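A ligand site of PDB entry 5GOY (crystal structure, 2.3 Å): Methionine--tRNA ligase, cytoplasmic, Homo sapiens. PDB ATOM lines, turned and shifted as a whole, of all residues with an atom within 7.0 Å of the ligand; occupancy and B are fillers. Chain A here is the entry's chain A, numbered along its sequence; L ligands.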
ATOM      1  N   SER A  52      -7.900  -6.218  -3.640  1.00  0.00           N
ATOM      2  CA  SER A  52      -7.075  -5.134  -3.130  1.00  0.00           C
ATOM      3  C   SER A  52      -7.657  -3.835  -3.642  1.00  0.00           C
ATOM      4  O   SER A  52      -8.183  -3.780  -4.750  1.00  0.00           O
ATOM      5  CB  SER A  52      -5.623  -5.286  -3.576  1.00  0.00           C
ATOM      6  OG  SER A  52      -4.865  -4.159  -3.177  1.00  0.00           O
ATOM      7  N   ALA A  53      -7.574  -2.787  -2.823  1.00  0.00           N
ATOM      8  CA  ALA A  53      -8.089  -1.477  -3.206  1.00  0.00           C
ATOM      9  C   ALA A  53      -7.459  -1.019  -4.515  1.00  0.00           C
ATOM     10  O   ALA A  53      -6.244  -1.074  -4.680  1.00  0.00           O
ATOM     11  CB  ALA A  53      -7.823  -0.470  -2.104  1.00  0.00           C
ATOM     12  N   LEU A  54      -8.305  -0.574  -5.445  1.00  0.00           N
ATOM     13  CA  LEU A  54      -7.862  -0.200  -6.781  1.00  0.00           C
ATOM     14  C   LEU A  54      -7.092   1.120  -6.753  1.00  0.00           C
ATOM     15  O   LEU A  54      -7.680   2.182  -6.542  1.00  0.00           O
ATOM     16  CB  LEU A  54      -9.051  -0.079  -7.731  1.00  0.00           C
ATOM     17  CG  LEU A  54     -10.071  -1.231  -7.710  1.00  0.00           C
ATOM     18  CD1 LEU A  54     -11.288  -0.876  -8.544  1.00  0.00           C
ATOM     19  CD2 LEU A  54      -9.439  -2.518  -8.190  1.00  0.00           C
ATOM     20  N   PRO A  55      -5.771   1.070  -6.976  1.00  0.00           N
ATOM     21  CA  PRO A  55      -4.954   2.286  -6.911  1.00  0.00           C
ATOM     22  C   PRO A  55      -5.330   3.285  -7.988  1.00  0.00           C
ATOM     23  O   PRO A  55      -5.605   2.882  -9.125  1.00  0.00           O
ATOM     24  CB  PRO A  55      -3.533   1.771  -7.126  1.00  0.00           C
ATOM     25  CG  PRO A  55      -3.709   0.513  -7.894  1.00  0.00           C
ATOM     26  CD  PRO A  55      -4.981  -0.103  -7.386  1.00  0.00           C
ATOM     27  N   TYR A  56      -5.371   4.569  -7.640  1.00  0.00           N
ATOM     28  CA  TYR A  56      -5.630   5.609  -8.619  1.00  0.00           C
ATOM     29  C   TYR A  56      -4.546   5.555  -9.697  1.00  0.00           C
ATOM     30  O   TYR A  56      -3.360   5.610  -9.388  1.00  0.00           O
ATOM     31  CB  TYR A  56      -5.692   6.980  -7.964  1.00  0.00           C
ATOM     32  CG  TYR A  56      -5.769   8.120  -8.955  1.00  0.00           C
ATOM     33  CD1 TYR A  56      -6.916   8.329  -9.709  1.00  0.00           C
ATOM     34  CD2 TYR A  56      -4.704   8.980  -9.137  1.00  0.00           C
ATOM     35  CE1 TYR A  56      -6.991   9.363 -10.624  1.00  0.00           C
ATOM     36  CE2 TYR A  56      -4.757  10.015 -10.042  1.00  0.00           C
ATOM     37  CZ  TYR A  56      -5.910  10.202 -10.789  1.00  0.00           C
ATOM     38  OH  TYR A  56      -5.977  11.232 -11.694  1.00  0.00           O
ATOM     39  N   VAL A  57      -4.966   5.451 -10.951  1.00  0.00           N
ATOM     40  CA  VAL A  57      -4.049   5.110 -12.039  1.00  0.00           C
ATOM     41  C   VAL A  57      -2.943   6.140 -12.290  1.00  0.00           C
ATOM     42  O   VAL A  57      -1.813   5.773 -12.601  1.00  0.00           O
ATOM     43  CB  VAL A  57      -4.829   4.863 -13.357  1.00  0.00           C
ATOM     44  CG1 VAL A  57      -5.523   6.134 -13.833  1.00  0.00           C
ATOM     45  CG2 VAL A  57      -3.898   4.312 -14.436  1.00  0.00           C
ATOM     46  N   ASN A  65       1.803   2.668  -0.345  1.00  0.00           N
ATOM     47  CA  ASN A  65       0.630   2.191  -1.064  1.00  0.00           C
ATOM     48  C   ASN A  65       0.677   0.688  -1.257  1.00  0.00           C
ATOM     49  O   ASN A  65      -0.334   0.000  -1.096  1.00  0.00           O
ATOM     50  CB  ASN A  65       0.525   2.876  -2.423  1.00  0.00           C
ATOM     51  CG  ASN A  65       0.421   4.378  -2.316  1.00  0.00           C
ATOM     52  OD1 ASN A  65       1.259   5.109  -2.842  1.00  0.00           O
ATOM     53  ND2 ASN A  65      -0.611   4.850  -1.629  1.00  0.00           N
ATOM     54  N   GLY A  92      -6.861  -3.828  -9.913  1.00  0.00           N
ATOM     55  CA  GLY A  92      -6.916  -3.070 -11.145  1.00  0.00           C
ATOM     56  C   GLY A  92      -6.818  -1.593 -10.872  1.00  0.00           C
ATOM     57  O   GLY A  92      -6.746  -1.178  -9.714  1.00  0.00           O
ATOM     58  N   THR A  93      -6.816  -0.782 -11.922  1.00  0.00           N
ATOM     59  CA  THR A  93      -6.598   0.650 -11.757  1.00  0.00           C
ATOM     60  C   THR A  93      -7.907   1.435 -11.710  1.00  0.00           C
ATOM     61  O   THR A  93      -8.816   1.222 -12.507  1.00  0.00           O
ATOM     62  CB  THR A  93      -5.712   1.216 -12.877  1.00  0.00           C
ATOM     63  OG1 THR A  93      -6.161   0.724 -14.149  1.00  0.00           O
ATOM     64  CG2 THR A  93      -4.259   0.776 -12.672  1.00  0.00           C
ATOM     65  N   ASP A  94      -7.978   2.339 -10.737  1.00  0.00           N
ATOM     66  CA  ASP A  94      -9.068   3.314 -10.605  1.00  0.00           C
ATOM     67  C   ASP A  94      -8.750   4.504 -11.508  1.00  0.00           C
ATOM     68  O   ASP A  94      -7.760   5.214 -11.269  1.00  0.00           O
ATOM     69  CB  ASP A  94      -9.216   3.738  -9.146  1.00  0.00           C
ATOM     70  CG  ASP A  94     -10.469   4.554  -8.888  1.00  0.00           C
ATOM     71  OD1 ASP A  94     -11.058   5.084  -9.850  1.00  0.00           O
ATOM     72  OD2 ASP A  94     -10.849   4.667  -7.709  1.00  0.00           O
ATOM     73  N   GLU A  95      -9.570   4.737 -12.526  1.00  0.00           N
ATOM     74  CA  GLU A  95      -9.161   5.619 -13.614  1.00  0.00           C
ATOM     75  C   GLU A  95     -10.039   6.855 -13.843  1.00  0.00           C
ATOM     76  O   GLU A  95      -9.563   7.881 -14.325  1.00  0.00           O
ATOM     77  CB  GLU A  95      -9.061   4.820 -14.909  1.00  0.00           C
ATOM     78  CG  GLU A  95      -8.139   3.618 -14.798  1.00  0.00           C
ATOM     79  CD  GLU A  95      -7.976   2.872 -16.109  1.00  0.00           C
ATOM     80  OE1 GLU A  95      -7.599   1.689 -16.062  1.00  0.00           O
ATOM     81  OE2 GLU A  95      -8.220   3.481 -17.168  1.00  0.00           O
ATOM     82  N   THR A 139     -11.176   0.096 -14.663  1.00  0.00           N
ATOM     83  CA  THR A 139     -12.528   0.567 -14.397  1.00  0.00           C
ATOM     84  C   THR A 139     -13.162   1.267 -15.595  1.00  0.00           C
ATOM     85  O   THR A 139     -14.331   1.657 -15.550  1.00  0.00           O
ATOM     86  CB  THR A 139     -12.551   1.542 -13.189  1.00  0.00           C
ATOM     87  OG1 THR A 139     -11.631   2.621 -13.430  1.00  0.00           O
ATOM     88  CG2 THR A 139     -12.153   0.817 -11.917  1.00  0.00           C
ATOM     89  N   VAL A 299     -17.093   9.079  -8.943  1.00  0.00           N
ATOM     90  CA  VAL A 299     -16.113   7.990  -8.946  1.00  0.00           C
ATOM     91  C   VAL A 299     -16.262   7.022  -7.782  1.00  0.00           C
ATOM     92  O   VAL A 299     -16.263   5.812  -7.973  1.00  0.00           O
ATOM     93  CB  VAL A 299     -14.667   8.526  -8.932  1.00  0.00           C
ATOM     94  CG1 VAL A 299     -14.242   8.876 -10.337  1.00  0.00           C
ATOM     95  CG2 VAL A 299     -14.541   9.727  -8.007  1.00  0.00           C
ATOM     96  N   TRP A 300     -16.401   7.561  -6.575  1.00  0.00           N
ATOM     97  CA  TRP A 300     -16.432   6.716  -5.389  1.00  0.00           C
ATOM     98  C   TRP A 300     -17.776   6.021  -5.192  1.00  0.00           C
ATOM     99  O   TRP A 300     -17.938   5.220  -4.272  1.00  0.00           O
ATOM    100  CB  TRP A 300     -16.086   7.547  -4.149  1.00  0.00           C
ATOM    101  CG  TRP A 300     -14.694   7.313  -3.648  1.00  0.00           C
ATOM    102  CD1 TRP A 300     -13.728   8.255  -3.413  1.00  0.00           C
ATOM    103  CD2 TRP A 300     -14.106   6.051  -3.300  1.00  0.00           C
ATOM    104  NE1 TRP A 300     -12.577   7.657  -2.953  1.00  0.00           N
ATOM    105  CE2 TRP A 300     -12.780   6.300  -2.876  1.00  0.00           C
ATOM    106  CE3 TRP A 300     -14.564   4.731  -3.311  1.00  0.00           C
ATOM    107  CZ2 TRP A 300     -11.920   5.287  -2.456  1.00  0.00           C
ATOM    108  CZ3 TRP A 300     -13.705   3.722  -2.907  1.00  0.00           C
ATOM    109  CH2 TRP A 300     -12.403   4.010  -2.479  1.00  0.00           C
ATOM    110  N   ASP A 302     -19.072   4.311  -7.919  1.00  0.00           N
ATOM    111  CA  ASP A 302     -18.931   3.145  -8.787  1.00  0.00           C
ATOM    112  C   ASP A 302     -17.510   2.580  -8.847  1.00  0.00           C
ATOM    113  O   ASP A 302     -17.258   1.617  -9.555  1.00  0.00           O
ATOM    114  CB  ASP A 302     -19.398   3.481 -10.206  1.00  0.00           C
ATOM    115  CG  ASP A 302     -18.378   4.274 -10.996  1.00  0.00           C
ATOM    116  OD1 ASP A 302     -17.809   5.229 -10.424  1.00  0.00           O
ATOM    117  OD2 ASP A 302     -18.138   3.938 -12.166  1.00  0.00           O
ATOM    118  N   ALA A 303     -16.587   3.183  -8.095  1.00  0.00           N
ATOM    119  CA  ALA A 303     -15.229   2.650  -8.025  1.00  0.00           C
ATOM    120  C   ALA A 303     -15.245   1.258  -7.409  1.00  0.00           C
ATOM    121  O   ALA A 303     -14.538   0.358  -7.862  1.00  0.00           O
ATOM    122  CB  ALA A 303     -14.325   3.567  -7.221  1.00  0.00           C
ATOM    123  N   THR A 304     -16.068   1.101  -6.385  1.00  0.00           N
ATOM    124  CA  THR A 304     -16.202  -0.174  -5.687  1.00  0.00           C
ATOM    125  C   THR A 304     -16.943  -1.191  -6.548  1.00  0.00           C
ATOM    126  O   THR A 304     -16.835  -2.403  -6.325  1.00  0.00           O
ATOM    127  CB  THR A 304     -16.951   0.012  -4.354  1.00  0.00           C
ATOM    128  OG1 THR A 304     -17.338  -1.263  -3.837  1.00  0.00           O
ATOM    129  CG2 THR A 304     -18.189   0.867  -4.563  1.00  0.00           C
ATOM    130  N   ILE A 305     -17.692  -0.698  -7.532  1.00  0.00           N
ATOM    131  CA  ILE A 305     -18.361  -1.561  -8.505  1.00  0.00           C
ATOM    132  C   ILE A 305     -17.317  -2.116  -9.479  1.00  0.00           C
ATOM    133  O   ILE A 305     -17.514  -3.165 -10.090  1.00  0.00           O
ATOM    134  CB  ILE A 305     -19.472  -0.790  -9.240  1.00  0.00           C
ATOM    135  CG1 ILE A 305     -20.623  -0.482  -8.265  1.00  0.00           C
ATOM    136  CG2 ILE A 305     -20.018  -1.580 -10.423  1.00  0.00           C
ATOM    137  CD1 ILE A 305     -21.606   0.544  -8.788  1.00  0.00           C
ATOM    138  N   GLY A 306     -16.186  -1.412  -9.571  1.00  0.00           N
ATOM    139  CA  GLY A 306     -15.062  -1.859 -10.364  1.00  0.00           C
ATOM    140  C   GLY A 306     -14.609  -3.278 -10.045  1.00  0.00           C
ATOM    141  O   GLY A 306     -14.232  -4.020 -10.939  1.00  0.00           O
ATOM    142  N   TYR A 307     -14.672  -3.647  -8.767  1.00  0.00           N
ATOM    143  CA  TYR A 307     -14.356  -5.017  -8.345  1.00  0.00           C
ATOM    144  C   TYR A 307     -15.153  -6.031  -9.148  1.00  0.00           C
ATOM    145  O   TYR A 307     -14.633  -7.057  -9.566  1.00  0.00           O
ATOM    146  CB  TYR A 307     -14.640  -5.209  -6.857  1.00  0.00           C
ATOM    147  CG  TYR A 307     -13.771  -4.407  -5.912  1.00  0.00           C
ATOM    148  CD1 TYR A 307     -12.391  -4.424  -6.030  1.00  0.00           C
ATOM    149  CD2 TYR A 307     -14.333  -3.649  -4.895  1.00  0.00           C
ATOM    150  CE1 TYR A 307     -11.601  -3.686  -5.167  1.00  0.00           C
ATOM    151  CE2 TYR A 307     -13.556  -2.917  -4.032  1.00  0.00           C
ATOM    152  CZ  TYR A 307     -12.182  -2.935  -4.174  1.00  0.00           C
ATOM    153  OH  TYR A 307     -11.412  -2.203  -3.305  1.00  0.00           O
ATOM    154  N   MET A 334      -7.309  -2.803   2.061  1.00  0.00           N
ATOM    155  CA  MET A 334      -7.285  -1.395   1.722  1.00  0.00           C
ATOM    156  C   MET A 334      -6.587  -0.554   2.776  1.00  0.00           C
ATOM    157  O   MET A 334      -6.164  -1.055   3.820  1.00  0.00           O
ATOM    158  CB  MET A 334      -8.705  -0.868   1.529  1.00  0.00           C
ATOM    159  CG  MET A 334      -9.508  -0.811   2.823  1.00  0.00           C
ATOM    160  SD  MET A 334     -11.276  -0.857   2.516  1.00  0.00           S
ATOM    161  CE  MET A 334     -11.428  -2.513   1.871  1.00  0.00           C
ATOM    162  N   ALA A 335      -6.466   0.736   2.503  1.00  0.00           N
ATOM    163  CA  ALA A 335      -5.976   1.684   3.483  1.00  0.00           C
ATOM    164  C   ALA A 335      -7.146   2.267   4.257  1.00  0.00           C
ATOM    165  O   ALA A 335      -8.286   2.246   3.770  1.00  0.00           O
ATOM    166  CB  ALA A 335      -5.164   2.782   2.813  1.00  0.00           C
ATOM    167  N   ASP A 337      -8.432   5.142   4.809  1.00  0.00           N
ATOM    168  CA  ASP A 337      -9.299   6.116   4.143  1.00  0.00           C
ATOM    169  C   ASP A 337     -10.337   5.489   3.219  1.00  0.00           C
ATOM    170  O   ASP A 337     -11.319   6.134   2.856  1.00  0.00           O
ATOM    171  CB  ASP A 337      -8.442   7.110   3.351  1.00  0.00           C
ATOM    172  CG  ASP A 337      -7.456   6.428   2.427  1.00  0.00           C
ATOM    173  OD1 ASP A 337      -7.334   5.191   2.495  1.00  0.00           O
ATOM    174  OD2 ASP A 337      -6.799   7.138   1.634  1.00  0.00           O
ATOM    175  N   ASN A 338     -10.130   4.232   2.837  1.00  0.00           N
ATOM    176  CA  ASN A 338     -11.027   3.536   1.925  1.00  0.00           C
ATOM    177  C   ASN A 338     -12.182   2.820   2.634  1.00  0.00           C
ATOM    178  O   ASN A 338     -13.186   2.488   1.999  1.00  0.00           O
ATOM    179  CB  ASN A 338     -10.256   2.526   1.074  1.00  0.00           C
ATOM    180  CG  ASN A 338      -9.458   3.177  -0.039  1.00  0.00           C
ATOM    181  OD1 ASN A 338      -9.281   4.400  -0.058  1.00  0.00           O
ATOM    182  ND2 ASN A 338      -8.978   2.368  -0.968  1.00  0.00           N
ATOM    183  N   PHE A 341     -16.145   3.520   2.241  1.00  0.00           N
ATOM    184  CA  PHE A 341     -16.751   3.177   0.972  1.00  0.00           C
ATOM    185  C   PHE A 341     -16.982   1.678   0.851  1.00  0.00           C
ATOM    186  O   PHE A 341     -17.863   1.234   0.110  1.00  0.00           O
ATOM    187  CB  PHE A 341     -15.885   3.660  -0.191  1.00  0.00           C
ATOM    188  CG  PHE A 341     -15.737   5.154  -0.250  1.00  0.00           C
ATOM    189  CD1 PHE A 341     -16.786   5.955  -0.674  1.00  0.00           C
ATOM    190  CD2 PHE A 341     -14.544   5.761   0.106  1.00  0.00           C
ATOM    191  CE1 PHE A 341     -16.659   7.327  -0.731  1.00  0.00           C
ATOM    192  CE2 PHE A 341     -14.403   7.138   0.049  1.00  0.00           C
ATOM    193  CZ  PHE A 341     -15.467   7.920  -0.378  1.00  0.00           C
ATOM    194  N   HIS A 342     -16.203   0.897   1.593  1.00  0.00           N
ATOM    195  CA  HIS A 342     -16.287  -0.556   1.527  1.00  0.00           C
ATOM    196  C   HIS A 342     -17.157  -1.139   2.649  1.00  0.00           C
ATOM    197  O   HIS A 342     -17.653  -2.258   2.521  1.00  0.00           O
ATOM    198  CB  HIS A 342     -14.890  -1.164   1.577  1.00  0.00           C
ATOM    199  CG  HIS A 342     -14.039  -0.835   0.390  1.00  0.00           C
ATOM    200  ND1 HIS A 342     -13.499   0.413   0.183  1.00  0.00           N
ATOM    201  CD2 HIS A 342     -13.625  -1.601  -0.649  1.00  0.00           C
ATOM    202  CE1 HIS A 342     -12.797   0.404  -0.932  1.00  0.00           C
ATOM    203  NE2 HIS A 342     -12.858  -0.800  -1.463  1.00  0.00           N
HETATM  204  N1  LIG L   1      -8.241   4.492  -5.966  1.00  0.00           N
HETATM  205  C1  LIG L   1      -8.750   4.665  -4.610  1.00  0.00           C
HETATM  206  C2  LIG L   1      -7.646   5.162  -3.674  1.00  0.00           C
HETATM  207  O1  LIG L   1      -7.920   5.668  -2.587  1.00  0.00           O
HETATM  208  C3  LIG L   1      -9.329   3.357  -4.076  1.00  0.00           C
HETATM  209  C4  LIG L   1     -10.408   2.733  -4.955  1.00  0.00           C
HETATM  210  S1  LIG L   1     -10.950   1.130  -4.309  1.00  0.00           S
HETATM  211  C5  LIG L   1     -12.391   0.818  -5.346  1.00  0.00           C
HETATM  212  O2  LIG L   1      -6.458   5.071  -3.983  1.00  0.00           O
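The backbone carbonyl oxygen of Pro 55 is in hydrogen-bond range of the backbone NH of Asp 94 (2.9 Å). The side-chain carboxylate of Asp 337 lies close to the side-chain amide oxygen of Asn 338 (3.3 Å). O of Asp 94 is in hydrogen-bond range of N of Val 57 (2.8 Å). The side-chain sulfur (SD) of Met 334 lies within hydrogen-bond range of a ring nitrogen (ND1) of His 342 (3.5 Å). The backbone carbonyl oxygen of Asn 338 lies within hydrogen-bond range of a ring nitrogen (ND1) of His 342, at 2.8 Å. A ring nitrogen (NE2) of His 342 lies within hydrogen-bond range of the side-chain hydroxyl of Tyr 307.
N of Tyr 56 lies close to N1 of the ligand (3.3 Å). The backbone carbonyl oxygen of Leu 54 sits at hydrogen-bond distance from a nitrogen (N1) of the ligand, at 2.4 Å. The side-chain amide oxygen of Asn 338 sits close to an oxygen (O1) of the ligand (3.1 Å). The side-chain hydroxyl (OH) of Tyr 307 lies close to a sulfur (S1) of the ligand, at 3.5 Å. N of Leu 54 lies close to S1 of the ligand (3.3 Å). N1 of the ligand is in salt-bridge range of OD2 of Asp 94.
Residues that only touch the ligand: Pro 55 (3.7 Å), Trp 300 (3.4 Å), Ala 303 (3.3 Å), Thr 304 (3.8 Å) and His 342 (3.9 Å). Hydrophobic or aromatic side chains that line the ligand: Leu 54, Trp 300, Ala 303, Tyr 307 and His 342. Ten residues have an atom within 4 Å of the ligand: Leu 54, Pro 55, Tyr 56, Asp 94, Trp 300, Ala 303, Thr 304, Tyr 307, Asn 338 and His 342. Along chain A the residues within 4 Å of the ligand span positions 54 to 342. The nearest printed residue that does not touch the ligand is Ala 53 (4.02 Å).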
